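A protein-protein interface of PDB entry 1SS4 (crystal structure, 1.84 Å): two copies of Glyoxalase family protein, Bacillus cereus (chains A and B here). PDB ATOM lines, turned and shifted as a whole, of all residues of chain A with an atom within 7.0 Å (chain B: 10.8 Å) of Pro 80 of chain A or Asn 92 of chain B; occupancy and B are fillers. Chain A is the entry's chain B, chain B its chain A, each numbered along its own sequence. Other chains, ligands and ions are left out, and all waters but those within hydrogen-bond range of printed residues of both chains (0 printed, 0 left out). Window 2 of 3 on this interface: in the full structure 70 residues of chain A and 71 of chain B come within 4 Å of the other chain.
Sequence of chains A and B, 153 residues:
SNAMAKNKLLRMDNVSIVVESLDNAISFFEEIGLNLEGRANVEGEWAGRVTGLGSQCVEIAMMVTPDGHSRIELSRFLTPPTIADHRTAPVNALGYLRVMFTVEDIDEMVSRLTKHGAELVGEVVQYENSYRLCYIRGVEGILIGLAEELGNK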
ATOM      1  N   VAL A  18      18.440  17.672   1.149  1.00  0.00           N
ATOM      2  CA  VAL A  18      17.122  18.198   0.819  1.00  0.00           C
ATOM      3  C   VAL A  18      17.282  18.983  -0.474  1.00  0.00           C
ATOM      4  O   VAL A  18      18.120  19.890  -0.574  1.00  0.00           O
ATOM      5  CB  VAL A  18      16.558  19.115   1.943  1.00  0.00           C
ATOM      6  CG1 VAL A  18      15.248  19.772   1.475  1.00  0.00           C
ATOM      7  CG2 VAL A  18      16.275  18.272   3.219  1.00  0.00           C
ATOM      8  N   THR A  51      11.225  14.287  13.358  1.00  0.00           N
ATOM      9  CA  THR A  51      11.796  15.581  12.978  1.00  0.00           C
ATOM     10  C   THR A  51      11.368  16.766  13.834  1.00  0.00           C
ATOM     11  O   THR A  51      12.039  17.797  13.849  1.00  0.00           O
ATOM     12  CB  THR A  51      11.419  15.946  11.538  1.00  0.00           C
ATOM     13  OG1 THR A  51      10.006  16.152  11.476  1.00  0.00           O
ATOM     14  CG2 THR A  51      11.797  14.835  10.576  1.00  0.00           C
ATOM     15  N   LEU A  53       8.613  18.355  13.277  1.00  0.00           N
ATOM     16  CA  LEU A  53       7.860  19.245  12.401  1.00  0.00           C
ATOM     17  C   LEU A  53       6.352  19.050  12.513  1.00  0.00           C
ATOM     18  O   LEU A  53       5.587  19.974  12.253  1.00  0.00           O
ATOM     19  CB  LEU A  53       8.306  19.066  10.945  1.00  0.00           C
ATOM     20  CG  LEU A  53       9.782  19.424  10.705  1.00  0.00           C
ATOM     21  CD1 LEU A  53      10.136  19.224   9.232  1.00  0.00           C
ATOM     22  CD2 LEU A  53      10.031  20.855  11.152  1.00  0.00           C
ATOM     23  N   GLY A  54       5.930  17.847  12.893  1.00  0.00           N
ATOM     24  CA  GLY A  54       4.507  17.565  13.046  1.00  0.00           C
ATOM     25  C   GLY A  54       3.825  17.167  11.753  1.00  0.00           C
ATOM     26  O   GLY A  54       4.001  16.049  11.268  1.00  0.00           O
ATOM     27  N   SER A  55       3.026  18.070  11.196  1.00  0.00           N
ATOM     28  CA  SER A  55       2.350  17.788   9.940  1.00  0.00           C
ATOM     29  C   SER A  55       3.452  17.804   8.893  1.00  0.00           C
ATOM     30  O   SER A  55       3.942  18.875   8.519  1.00  0.00           O
ATOM     31  CB  SER A  55       1.325  18.878   9.628  1.00  0.00           C
ATOM     32  OG  SER A  55       0.745  18.674   8.349  1.00  0.00           O
ATOM     33  N   GLN A  56       3.848  16.623   8.426  1.00  0.00           N
ATOM     34  CA  GLN A  56       4.921  16.535   7.447  1.00  0.00           C
ATOM     35  C   GLN A  56       4.728  15.504   6.346  1.00  0.00           C
ATOM     36  O   GLN A  56       4.290  14.377   6.593  1.00  0.00           O
ATOM     37  CB  GLN A  56       6.247  16.259   8.165  1.00  0.00           C
ATOM     38  CG  GLN A  56       7.313  15.586   7.303  1.00  0.00           C
ATOM     39  CD  GLN A  56       8.602  15.318   8.055  1.00  0.00           C
ATOM     40  OE1 GLN A  56       9.407  14.485   7.648  1.00  0.00           O
ATOM     41  NE2 GLN A  56       8.810  16.033   9.151  1.00  0.00           N
ATOM     42  N   CYS A  57       5.065  15.914   5.129  1.00  0.00           N
ATOM     43  CA  CYS A  57       5.000  15.044   3.976  1.00  0.00           C
ATOM     44  C   CYS A  57       6.266  15.290   3.164  1.00  0.00           C
ATOM     45  O   CYS A  57       6.504  16.403   2.691  1.00  0.00           O
ATOM     46  CB  CYS A  57       3.785  15.342   3.121  1.00  0.00           C
ATOM     47  SG  CYS A  57       3.704  14.247   1.689  1.00  0.00           S
ATOM     48  N   VAL A  58       7.082  14.253   3.026  1.00  0.00           N
ATOM     49  CA  VAL A  58       8.324  14.358   2.283  1.00  0.00           C
ATOM     50  C   VAL A  58       8.445  13.213   1.281  1.00  0.00           C
ATOM     51  O   VAL A  58       8.043  12.090   1.571  1.00  0.00           O
ATOM     52  CB  VAL A  58       9.528  14.295   3.240  1.00  0.00           C
ATOM     53  CG1 VAL A  58      10.835  14.386   2.449  1.00  0.00           C
ATOM     54  CG2 VAL A  58       9.439  15.430   4.261  1.00  0.00           C
ATOM     55  N   PHE A  77      10.770  18.394   0.445  1.00  0.00           N
ATOM     56  CA  PHE A  77       9.688  18.692   1.378  1.00  0.00           C
ATOM     57  C   PHE A  77       8.428  19.184   0.675  1.00  0.00           C
ATOM     58  O   PHE A  77       8.502  20.077  -0.165  1.00  0.00           O
ATOM     59  CB  PHE A  77      10.146  19.751   2.388  1.00  0.00           C
ATOM     60  CG  PHE A  77      10.729  19.172   3.651  1.00  0.00           C
ATOM     61  CD1 PHE A  77       9.898  18.832   4.712  1.00  0.00           C
ATOM     62  CD2 PHE A  77      12.094  18.920   3.761  1.00  0.00           C
ATOM     63  CE1 PHE A  77      10.422  18.244   5.863  1.00  0.00           C
ATOM     64  CE2 PHE A  77      12.627  18.332   4.906  1.00  0.00           C
ATOM     65  CZ  PHE A  77      11.784  17.993   5.962  1.00  0.00           C
ATOM     66  N   LEU A  78       7.282  18.576   0.983  1.00  0.00           N
ATOM     67  CA  LEU A  78       6.024  19.055   0.418  1.00  0.00           C
ATOM     68  C   LEU A  78       5.399  19.857   1.558  1.00  0.00           C
ATOM     69  O   LEU A  78       4.956  20.989   1.372  1.00  0.00           O
ATOM     70  CB  LEU A  78       5.109  17.898  -0.007  1.00  0.00           C
ATOM     71  CG  LEU A  78       5.400  17.295  -1.390  1.00  0.00           C
ATOM     72  CD1 LEU A  78       6.663  16.442  -1.334  1.00  0.00           C
ATOM     73  CD2 LEU A  78       4.211  16.435  -1.841  1.00  0.00           C
ATOM     74  N   THR A  79       5.403  19.278   2.752  1.00  0.00           N
ATOM     75  CA  THR A  79       4.869  19.953   3.929  1.00  0.00           C
ATOM     76  C   THR A  79       5.732  19.620   5.133  1.00  0.00           C
ATOM     77  O   THR A  79       6.060  18.461   5.344  1.00  0.00           O
ATOM     78  CB  THR A  79       3.425  19.482   4.244  1.00  0.00           C
ATOM     79  OG1 THR A  79       2.591  19.715   3.109  1.00  0.00           O
ATOM     80  CG2 THR A  79       2.861  20.247   5.443  1.00  0.00           C
ATOM     81  N   PRO A  80       6.192  20.637   5.886  1.00  0.00           N
ATOM     82  CA  PRO A  80       5.956  22.071   5.657  1.00  0.00           C
ATOM     83  C   PRO A  80       6.937  22.483   4.573  1.00  0.00           C
ATOM     84  O   PRO A  80       7.943  21.800   4.376  1.00  0.00           O
ATOM     85  CB  PRO A  80       6.346  22.702   6.982  1.00  0.00           C
ATOM     86  CG  PRO A  80       7.462  21.805   7.474  1.00  0.00           C
ATOM     87  CD  PRO A  80       6.912  20.416   7.156  1.00  0.00           C
ATOM     88  N   PRO A  81       6.662  23.571   3.841  1.00  0.00           N
ATOM     89  CA  PRO A  81       7.653  23.929   2.819  1.00  0.00           C
ATOM     90  C   PRO A  81       8.993  24.341   3.480  1.00  0.00           C
ATOM     91  O   PRO A  81       9.042  24.643   4.689  1.00  0.00           O
ATOM     92  CB  PRO A  81       6.964  25.066   2.049  1.00  0.00           C
ATOM     93  CG  PRO A  81       6.020  25.652   3.050  1.00  0.00           C
ATOM     94  CD  PRO A  81       5.470  24.430   3.759  1.00  0.00           C
ATOM     95  N   THR A  82      10.085  24.339   2.718  1.00  0.00           N
ATOM     96  CA  THR A  82      11.374  24.720   3.297  1.00  0.00           C
ATOM     97  C   THR A  82      11.447  26.209   3.634  1.00  0.00           C
ATOM     98  O   THR A  82      10.834  27.049   2.967  1.00  0.00           O
ATOM     99  CB  THR A  82      12.558  24.336   2.381  1.00  0.00           C
ATOM    100  OG1 THR A  82      12.388  24.925   1.089  1.00  0.00           O
ATOM    101  CG2 THR A  82      12.638  22.816   2.254  1.00  0.00           C
ATOM    102  N   ILE A  83      12.195  26.527   4.682  1.00  0.00           N
ATOM    103  CA  ILE A  83      12.309  27.906   5.136  1.00  0.00           C
ATOM    104  C   ILE A  83      13.724  28.479   5.095  1.00  0.00           C
ATOM    105  O   ILE A  83      13.954  29.598   5.550  1.00  0.00           O
ATOM    106  CB  ILE A  83      11.747  28.069   6.561  1.00  0.00           C
ATOM    107  CG1 ILE A  83      12.484  27.128   7.520  1.00  0.00           C
ATOM    108  CG2 ILE A  83      10.230  27.770   6.552  1.00  0.00           C
ATOM    109  CD1 ILE A  83      12.065  27.291   9.017  1.00  0.00           C
ATOM    110  N   ALA A  84      14.668  27.714   4.554  1.00  0.00           N
ATOM    111  CA  ALA A  84      16.039  28.204   4.404  1.00  0.00           C
ATOM    112  C   ALA A  84      16.768  27.374   3.355  1.00  0.00           C
ATOM    113  O   ALA A  84      16.278  26.339   2.922  1.00  0.00           O
ATOM    114  CB  ALA A  84      16.773  28.156   5.713  1.00  0.00           C
ATOM    115  N   ASP A  85      17.958  27.822   2.985  1.00  0.00           N
ATOM    116  CA  ASP A  85      18.717  27.141   1.956  1.00  0.00           C
ATOM    117  C   ASP A  85      20.210  27.337   2.184  1.00  0.00           C
ATOM    118  O   ASP A  85      20.670  28.456   2.359  1.00  0.00           O
ATOM    119  CB  ASP A  85      18.275  27.728   0.611  1.00  0.00           C
ATOM    120  CG  ASP A  85      19.081  27.208  -0.572  1.00  0.00           C
ATOM    121  OD1 ASP A  85      19.720  26.142  -0.476  1.00  0.00           O
ATOM    122  OD2 ASP A  85      19.060  27.878  -1.619  1.00  0.00           O
ATOM    123  N   HIS B  86      25.612  26.853   8.913  1.00  0.00           N
ATOM    124  CA  HIS B  86      24.324  26.193   8.737  1.00  0.00           C
ATOM    125  C   HIS B  86      24.289  24.974   9.673  1.00  0.00           C
ATOM    126  O   HIS B  86      23.521  24.044   9.489  1.00  0.00           O
ATOM    127  CB  HIS B  86      24.043  25.774   7.276  1.00  0.00           C
ATOM    128  CG  HIS B  86      25.192  25.101   6.594  1.00  0.00           C
ATOM    129  ND1 HIS B  86      26.217  25.804   6.006  1.00  0.00           N
ATOM    130  CD2 HIS B  86      25.472  23.790   6.401  1.00  0.00           C
ATOM    131  CE1 HIS B  86      27.082  24.955   5.476  1.00  0.00           C
ATOM    132  NE2 HIS B  86      26.652  23.726   5.700  1.00  0.00           N
ATOM    133  N   THR B  88      23.090  24.751  12.596  1.00  0.00           N
ATOM    134  CA  THR B  88      21.783  24.615  13.225  1.00  0.00           C
ATOM    135  C   THR B  88      20.627  24.954  12.279  1.00  0.00           C
ATOM    136  O   THR B  88      19.593  25.454  12.703  1.00  0.00           O
ATOM    137  CB  THR B  88      21.704  25.474  14.532  1.00  0.00           C
ATOM    138  OG1 THR B  88      22.272  26.767  14.305  1.00  0.00           O
ATOM    139  CG2 THR B  88      22.489  24.792  15.671  1.00  0.00           C
ATOM    140  N   ALA B  89      20.807  24.679  10.991  1.00  0.00           N
ATOM    141  CA  ALA B  89      19.766  24.959  10.007  1.00  0.00           C
ATOM    142  C   ALA B  89      18.517  24.162  10.359  1.00  0.00           C
ATOM    143  O   ALA B  89      18.606  23.086  10.973  1.00  0.00           O
ATOM    144  CB  ALA B  89      20.251  24.561   8.597  1.00  0.00           C
ATOM    145  N   PRO B  90      17.339  24.684  10.011  1.00  0.00           N
ATOM    146  CA  PRO B  90      16.138  23.907  10.338  1.00  0.00           C
ATOM    147  C   PRO B  90      16.096  22.604   9.535  1.00  0.00           C
ATOM    148  O   PRO B  90      16.771  22.469   8.502  1.00  0.00           O
ATOM    149  CB  PRO B  90      14.986  24.850   9.986  1.00  0.00           C
ATOM    150  CG  PRO B  90      15.588  25.885   9.096  1.00  0.00           C
ATOM    151  CD  PRO B  90      17.008  26.047   9.561  1.00  0.00           C
ATOM    152  N   VAL B  91      15.323  21.637  10.020  1.00  0.00           N
ATOM    153  CA  VAL B  91      15.218  20.371   9.311  1.00  0.00           C
ATOM    154  C   VAL B  91      14.651  20.645   7.913  1.00  0.00           C
ATOM    155  O   VAL B  91      15.127  20.078   6.925  1.00  0.00           O
ATOM    156  CB  VAL B  91      14.294  19.387  10.058  1.00  0.00           C
ATOM    157  CG1 VAL B  91      14.082  18.138   9.224  1.00  0.00           C
ATOM    158  CG2 VAL B  91      14.897  19.036  11.424  1.00  0.00           C
ATOM    159  N   ASN B  92      13.642  21.513   7.829  1.00  0.00           N
ATOM    160  CA  ASN B  92      13.044  21.818   6.530  1.00  0.00           C
ATOM    161  C   ASN B  92      13.780  22.967   5.825  1.00  0.00           C
ATOM    162  O   ASN B  92      13.272  24.091   5.694  1.00  0.00           O
ATOM    163  CB  ASN B  92      11.522  22.108   6.677  1.00  0.00           C
ATOM    164  CG  ASN B  92      11.211  23.245   7.669  1.00  0.00           C
ATOM    165  OD1 ASN B  92      11.867  23.387   8.712  1.00  0.00           O
ATOM    166  ND2 ASN B  92      10.190  24.040   7.354  1.00  0.00           N
ATOM    167  N   ALA B  93      15.012  22.668   5.410  1.00  0.00           N
ATOM    168  CA  ALA B  93      15.864  23.617   4.697  1.00  0.00           C
ATOM    169  C   ALA B  93      16.539  22.862   3.574  1.00  0.00           C
ATOM    170  O   ALA B  93      16.787  21.665   3.680  1.00  0.00           O
ATOM    171  CB  ALA B  93      16.940  24.210   5.631  1.00  0.00           C
ATOM    172  N   LEU B  94      16.842  23.567   2.503  1.00  0.00           N
ATOM    173  CA  LEU B  94      17.502  22.962   1.355  1.00  0.00           C
ATOM    174  C   LEU B  94      18.997  22.774   1.612  1.00  0.00           C
ATOM    175  O   LEU B  94      19.642  23.638   2.207  1.00  0.00           O
ATOM    176  CB  LEU B  94      17.270  23.832   0.113  1.00  0.00           C
ATOM    177  CG  LEU B  94      15.797  23.927  -0.323  1.00  0.00           C
ATOM    178  CD1 LEU B  94      15.542  25.258  -1.031  1.00  0.00           C
ATOM    179  CD2 LEU B  94      15.434  22.731  -1.213  1.00  0.00           C
ATOM    180  N   GLY B  95      19.532  21.642   1.159  1.00  0.00           N
ATOM    181  CA  GLY B  95      20.948  21.346   1.336  1.00  0.00           C
ATOM    182  C   GLY B  95      21.190  20.117   2.215  1.00  0.00           C
ATOM    183  O   GLY B  95      20.248  19.428   2.615  1.00  0.00           O
ATOM    184  N   TYR B  96      22.461  19.824   2.485  1.00  0.00           N
ATOM    185  CA  TYR B  96      22.815  18.664   3.314  1.00  0.00           C
ATOM    186  C   TYR B  96      22.027  18.735   4.603  1.00  0.00           C
ATOM    187  O   TYR B  96      21.959  19.784   5.242  1.00  0.00           O
ATOM    188  CB  TYR B  96      24.315  18.653   3.604  1.00  0.00           C
ATOM    189  CG  TYR B  96      25.132  18.235   2.405  1.00  0.00           C
ATOM    190  CD1 TYR B  96      25.145  16.900   1.989  1.00  0.00           C
ATOM    191  CD2 TYR B  96      25.880  19.166   1.679  1.00  0.00           C
ATOM    192  CE1 TYR B  96      25.867  16.500   0.904  1.00  0.00           C
ATOM    193  CE2 TYR B  96      26.621  18.775   0.573  1.00  0.00           C
ATOM    194  CZ  TYR B  96      26.608  17.438   0.193  1.00  0.00           C
ATOM    195  OH  TYR B  96      27.341  16.998  -0.868  1.00  0.00           O
ATOM    196  N   LEU B  97      21.440  17.608   4.998  1.00  0.00           N
ATOM    197  CA  LEU B  97      20.609  17.588   6.202  1.00  0.00           C
ATOM    198  C   LEU B  97      21.215  16.845   7.383  1.00  0.00           C
ATOM    199  O   LEU B  97      21.457  17.423   8.461  1.00  0.00           O
ATOM    200  CB  LEU B  97      19.241  16.962   5.874  1.00  0.00           C
ATOM    201  CG  LEU B  97      18.255  16.863   7.040  1.00  0.00           C
ATOM    202  CD1 LEU B  97      17.932  18.238   7.550  1.00  0.00           C
ATOM    203  CD2 LEU B  97      16.955  16.144   6.598  1.00  0.00           C
ATOM    204  N   ARG B  98      21.446  15.556   7.199  1.00  0.00           N
ATOM    205  CA  ARG B  98      22.004  14.791   8.298  1.00  0.00           C
ATOM    206  C   ARG B  98      22.552  13.466   7.832  1.00  0.00           C
ATOM    207  O   ARG B  98      22.145  12.951   6.793  1.00  0.00           O
ATOM    208  CB  ARG B  98      20.896  14.518   9.326  1.00  0.00           C
ATOM    209  CG  ARG B  98      19.679  13.760   8.722  1.00  0.00           C
ATOM    210  CD  ARG B  98      19.680  12.309   9.152  1.00  0.00           C
ATOM    211  NE  ARG B  98      18.713  11.463   8.449  1.00  0.00           N
ATOM    212  CZ  ARG B  98      18.992  10.776   7.348  1.00  0.00           C
ATOM    213  NH1 ARG B  98      20.207  10.847   6.811  1.00  0.00           N
ATOM    214  NH2 ARG B  98      18.088   9.965   6.819  1.00  0.00           N
ATOM    215  N   VAL B 121      15.732  15.900  19.029  1.00  0.00           N
ATOM    216  CA  VAL B 121      14.932  16.845  18.256  1.00  0.00           C
ATOM    217  C   VAL B 121      13.449  16.609  18.406  1.00  0.00           C
ATOM    218  O   VAL B 121      12.679  17.555  18.579  1.00  0.00           O
ATOM    219  CB  VAL B 121      15.303  16.798  16.762  1.00  0.00           C
ATOM    220  CG1 VAL B 121      14.453  17.804  15.964  1.00  0.00           C
ATOM    221  CG2 VAL B 121      16.773  17.112  16.614  1.00  0.00           C
ATOM    222  N   TYR B 135      16.152  11.977  15.780  1.00  0.00           N
ATOM    223  CA  TYR B 135      17.076  12.993  15.285  1.00  0.00           C
ATOM    224  C   TYR B 135      17.640  13.623  16.540  1.00  0.00           C
ATOM    225  O   TYR B 135      16.915  13.874  17.502  1.00  0.00           O
ATOM    226  CB  TYR B 135      16.362  14.081  14.482  1.00  0.00           C
ATOM    227  CG  TYR B 135      16.165  13.795  13.011  1.00  0.00           C
ATOM    228  CD1 TYR B 135      15.736  14.809  12.145  1.00  0.00           C
ATOM    229  CD2 TYR B 135      16.381  12.528  12.485  1.00  0.00           C
ATOM    230  CE1 TYR B 135      15.531  14.560  10.797  1.00  0.00           C
ATOM    231  CE2 TYR B 135      16.171  12.266  11.144  1.00  0.00           C
ATOM    232  CZ  TYR B 135      15.744  13.290  10.305  1.00  0.00           C
ATOM    233  OH  TYR B 135      15.506  13.016   8.985  1.00  0.00           O
ATOM    234  N   ARG B 137      20.524  16.691  17.956  1.00  0.00           N
ATOM    235  CA  ARG B 137      21.390  17.824  17.673  1.00  0.00           C
ATOM    236  C   ARG B 137      22.615  17.478  18.525  1.00  0.00           C
ATOM    237  O   ARG B 137      22.553  17.496  19.770  1.00  0.00           O
ATOM    238  CB  ARG B 137      20.766  19.137  18.161  1.00  0.00           C
ATOM    239  CG  ARG B 137      19.563  19.604  17.358  1.00  0.00           C
ATOM    240  CD  ARG B 137      19.951  20.701  16.399  1.00  0.00           C
ATOM    241  NE  ARG B 137      18.899  21.027  15.436  1.00  0.00           N
ATOM    242  CZ  ARG B 137      19.148  21.363  14.176  1.00  0.00           C
ATOM    243  NH1 ARG B 137      20.406  21.403  13.764  1.00  0.00           N
ATOM    244  NH2 ARG B 137      18.154  21.662  13.335  1.00  0.00           N
ATOM    245  N   LEU B 143      23.018  18.267  13.164  1.00  0.00           N
ATOM    246  CA  LEU B 143      21.970  17.260  13.047  1.00  0.00           C
ATOM    247  C   LEU B 143      22.468  15.872  12.641  1.00  0.00           C
ATOM    248  O   LEU B 143      23.133  15.705  11.610  1.00  0.00           O
ATOM    249  CB  LEU B 143      20.913  17.728  12.047  1.00  0.00           C
ATOM    250  CG  LEU B 143      19.608  16.927  12.008  1.00  0.00           C
ATOM    251  CD1 LEU B 143      18.867  17.131  13.325  1.00  0.00           C
ATOM    252  CD2 LEU B 143      18.741  17.412  10.825  1.00  0.00           C
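Pro 80 of chain A touches just one residue of chain B: Asn 92.
Of chain A, only Leu 53, Phe 77, Pro 80, Pro 81, Thr 82 and Ile 83 come within 4 Å of Asn 92 of chain B.
Of chain B, only Asn 92 (3.0 Å) comes within 4 Å of Pro 81 of chain A.
Of chain B, only Asn 92 (3.1 Å), Ala 93 (3.95 Å) and Leu 94 (3.8 Å) come within 4 Å of Thr 82 of chain A.
Of chain B, only Ala 93 and Leu 94 come within 4 Å of Ala 84 of chain A.
Of the printed residues of chain A, Ala 93 of chain B touches Val 18, Thr 82 and Ala 84.
Printed residues of chain B within 4 Å of Val 18 of chain A: Ala 93, Leu 94 and Gly 95.
Printed residues of chain A within 4 Å of Tyr 135 of chain B: Thr 51.
Of the printed residues of chain A, Val 91 of chain B touches Thr 51 (3.9 Å) and Phe 77 (3.7 Å).
Printed residues of chain A within 4 Å of Gly 95 of chain B: Val 18 (2.8 Å).
The nearest residue of chain B that does not touch Pro 80 of chain A is Ala 93 of chain B (7.2 Å).
Ala 93 of chain B touches Val 18 of chain A.
Thr 51 of chain A touches Tyr 135 of chain B.
Asn 92 of chain B touches Leu 53 of chain A.
Phe 77 of chain A touches Val 91 of chain B (CE2 to O, 3.7 Å).
CE2 of Phe 77 of chain A touches CA of Asn 92 of chain B, 3.9 Å away.
CA of Thr 82 of chain A touches O of Asn 92 of chain B, 3.1 Å away.
CG2 of Thr 82 of chain A touches N of Ala 93 of chain B, 3.95 Å away.
Ile 83 of chain A touches Pro 90 of chain B (CG1 to CG, 3.7 Å).
O of Ala 84 of chain A touches CA of Ala 93 of chain B, at 3.3 Å.
Leu 94 of chain B touches Asp 85 of chain A.
Printed residues of chain A that touch a printed residue of chain B: Val 18, Thr 51, Leu 53, Phe 77, Pro 80, Pro 81, Thr 82, Ile 83, Ala 84 and Asp 85.
Along chain A the printed residues that touch a printed residue of chain B span positions 18 to 85.
Printed residues of chain B that touch a printed residue of chain A: Pro 90, Val 91, Asn 92, Ala 93, Leu 94, Gly 95, Val 121 and Tyr 135.
Hydrophobic or aromatic side chains of chain B that line the printed part of chain A: Pro 90, Val 91, Ala 93, Leu 94, Val 121 and Tyr 135.
O of Tyr 135 of chain B sits at hydrogen-bond distance from N of Val 121 of chain B (2.8 Å).
OG1 of Thr 51 of chain A lies within hydrogen-bond range of N of Leu 53 of chain A (3.2 Å).
NE2 of Gln 56 of chain A lies within hydrogen-bond range of OG1 of Thr 51 of chain A (2.6 Å).
ND2 of Asn 92 of chain B is in hydrogen-bond range of O of Pro 81 of chain A (3.0 Å).
O of Asn 92 of chain B is in hydrogen-bond range of N of Ile 83 of chain A (2.8 Å).
The backbone carbonyl oxygen (O) of Ala 84 of chain A sits at hydrogen-bond distance from the backbone NH (N) of Leu 94 of chain B.
The backbone NH of Gly 95 of chain B lies within hydrogen-bond range of the backbone carbonyl oxygen of Val 18 of chain A.
No position is printed for both chains.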
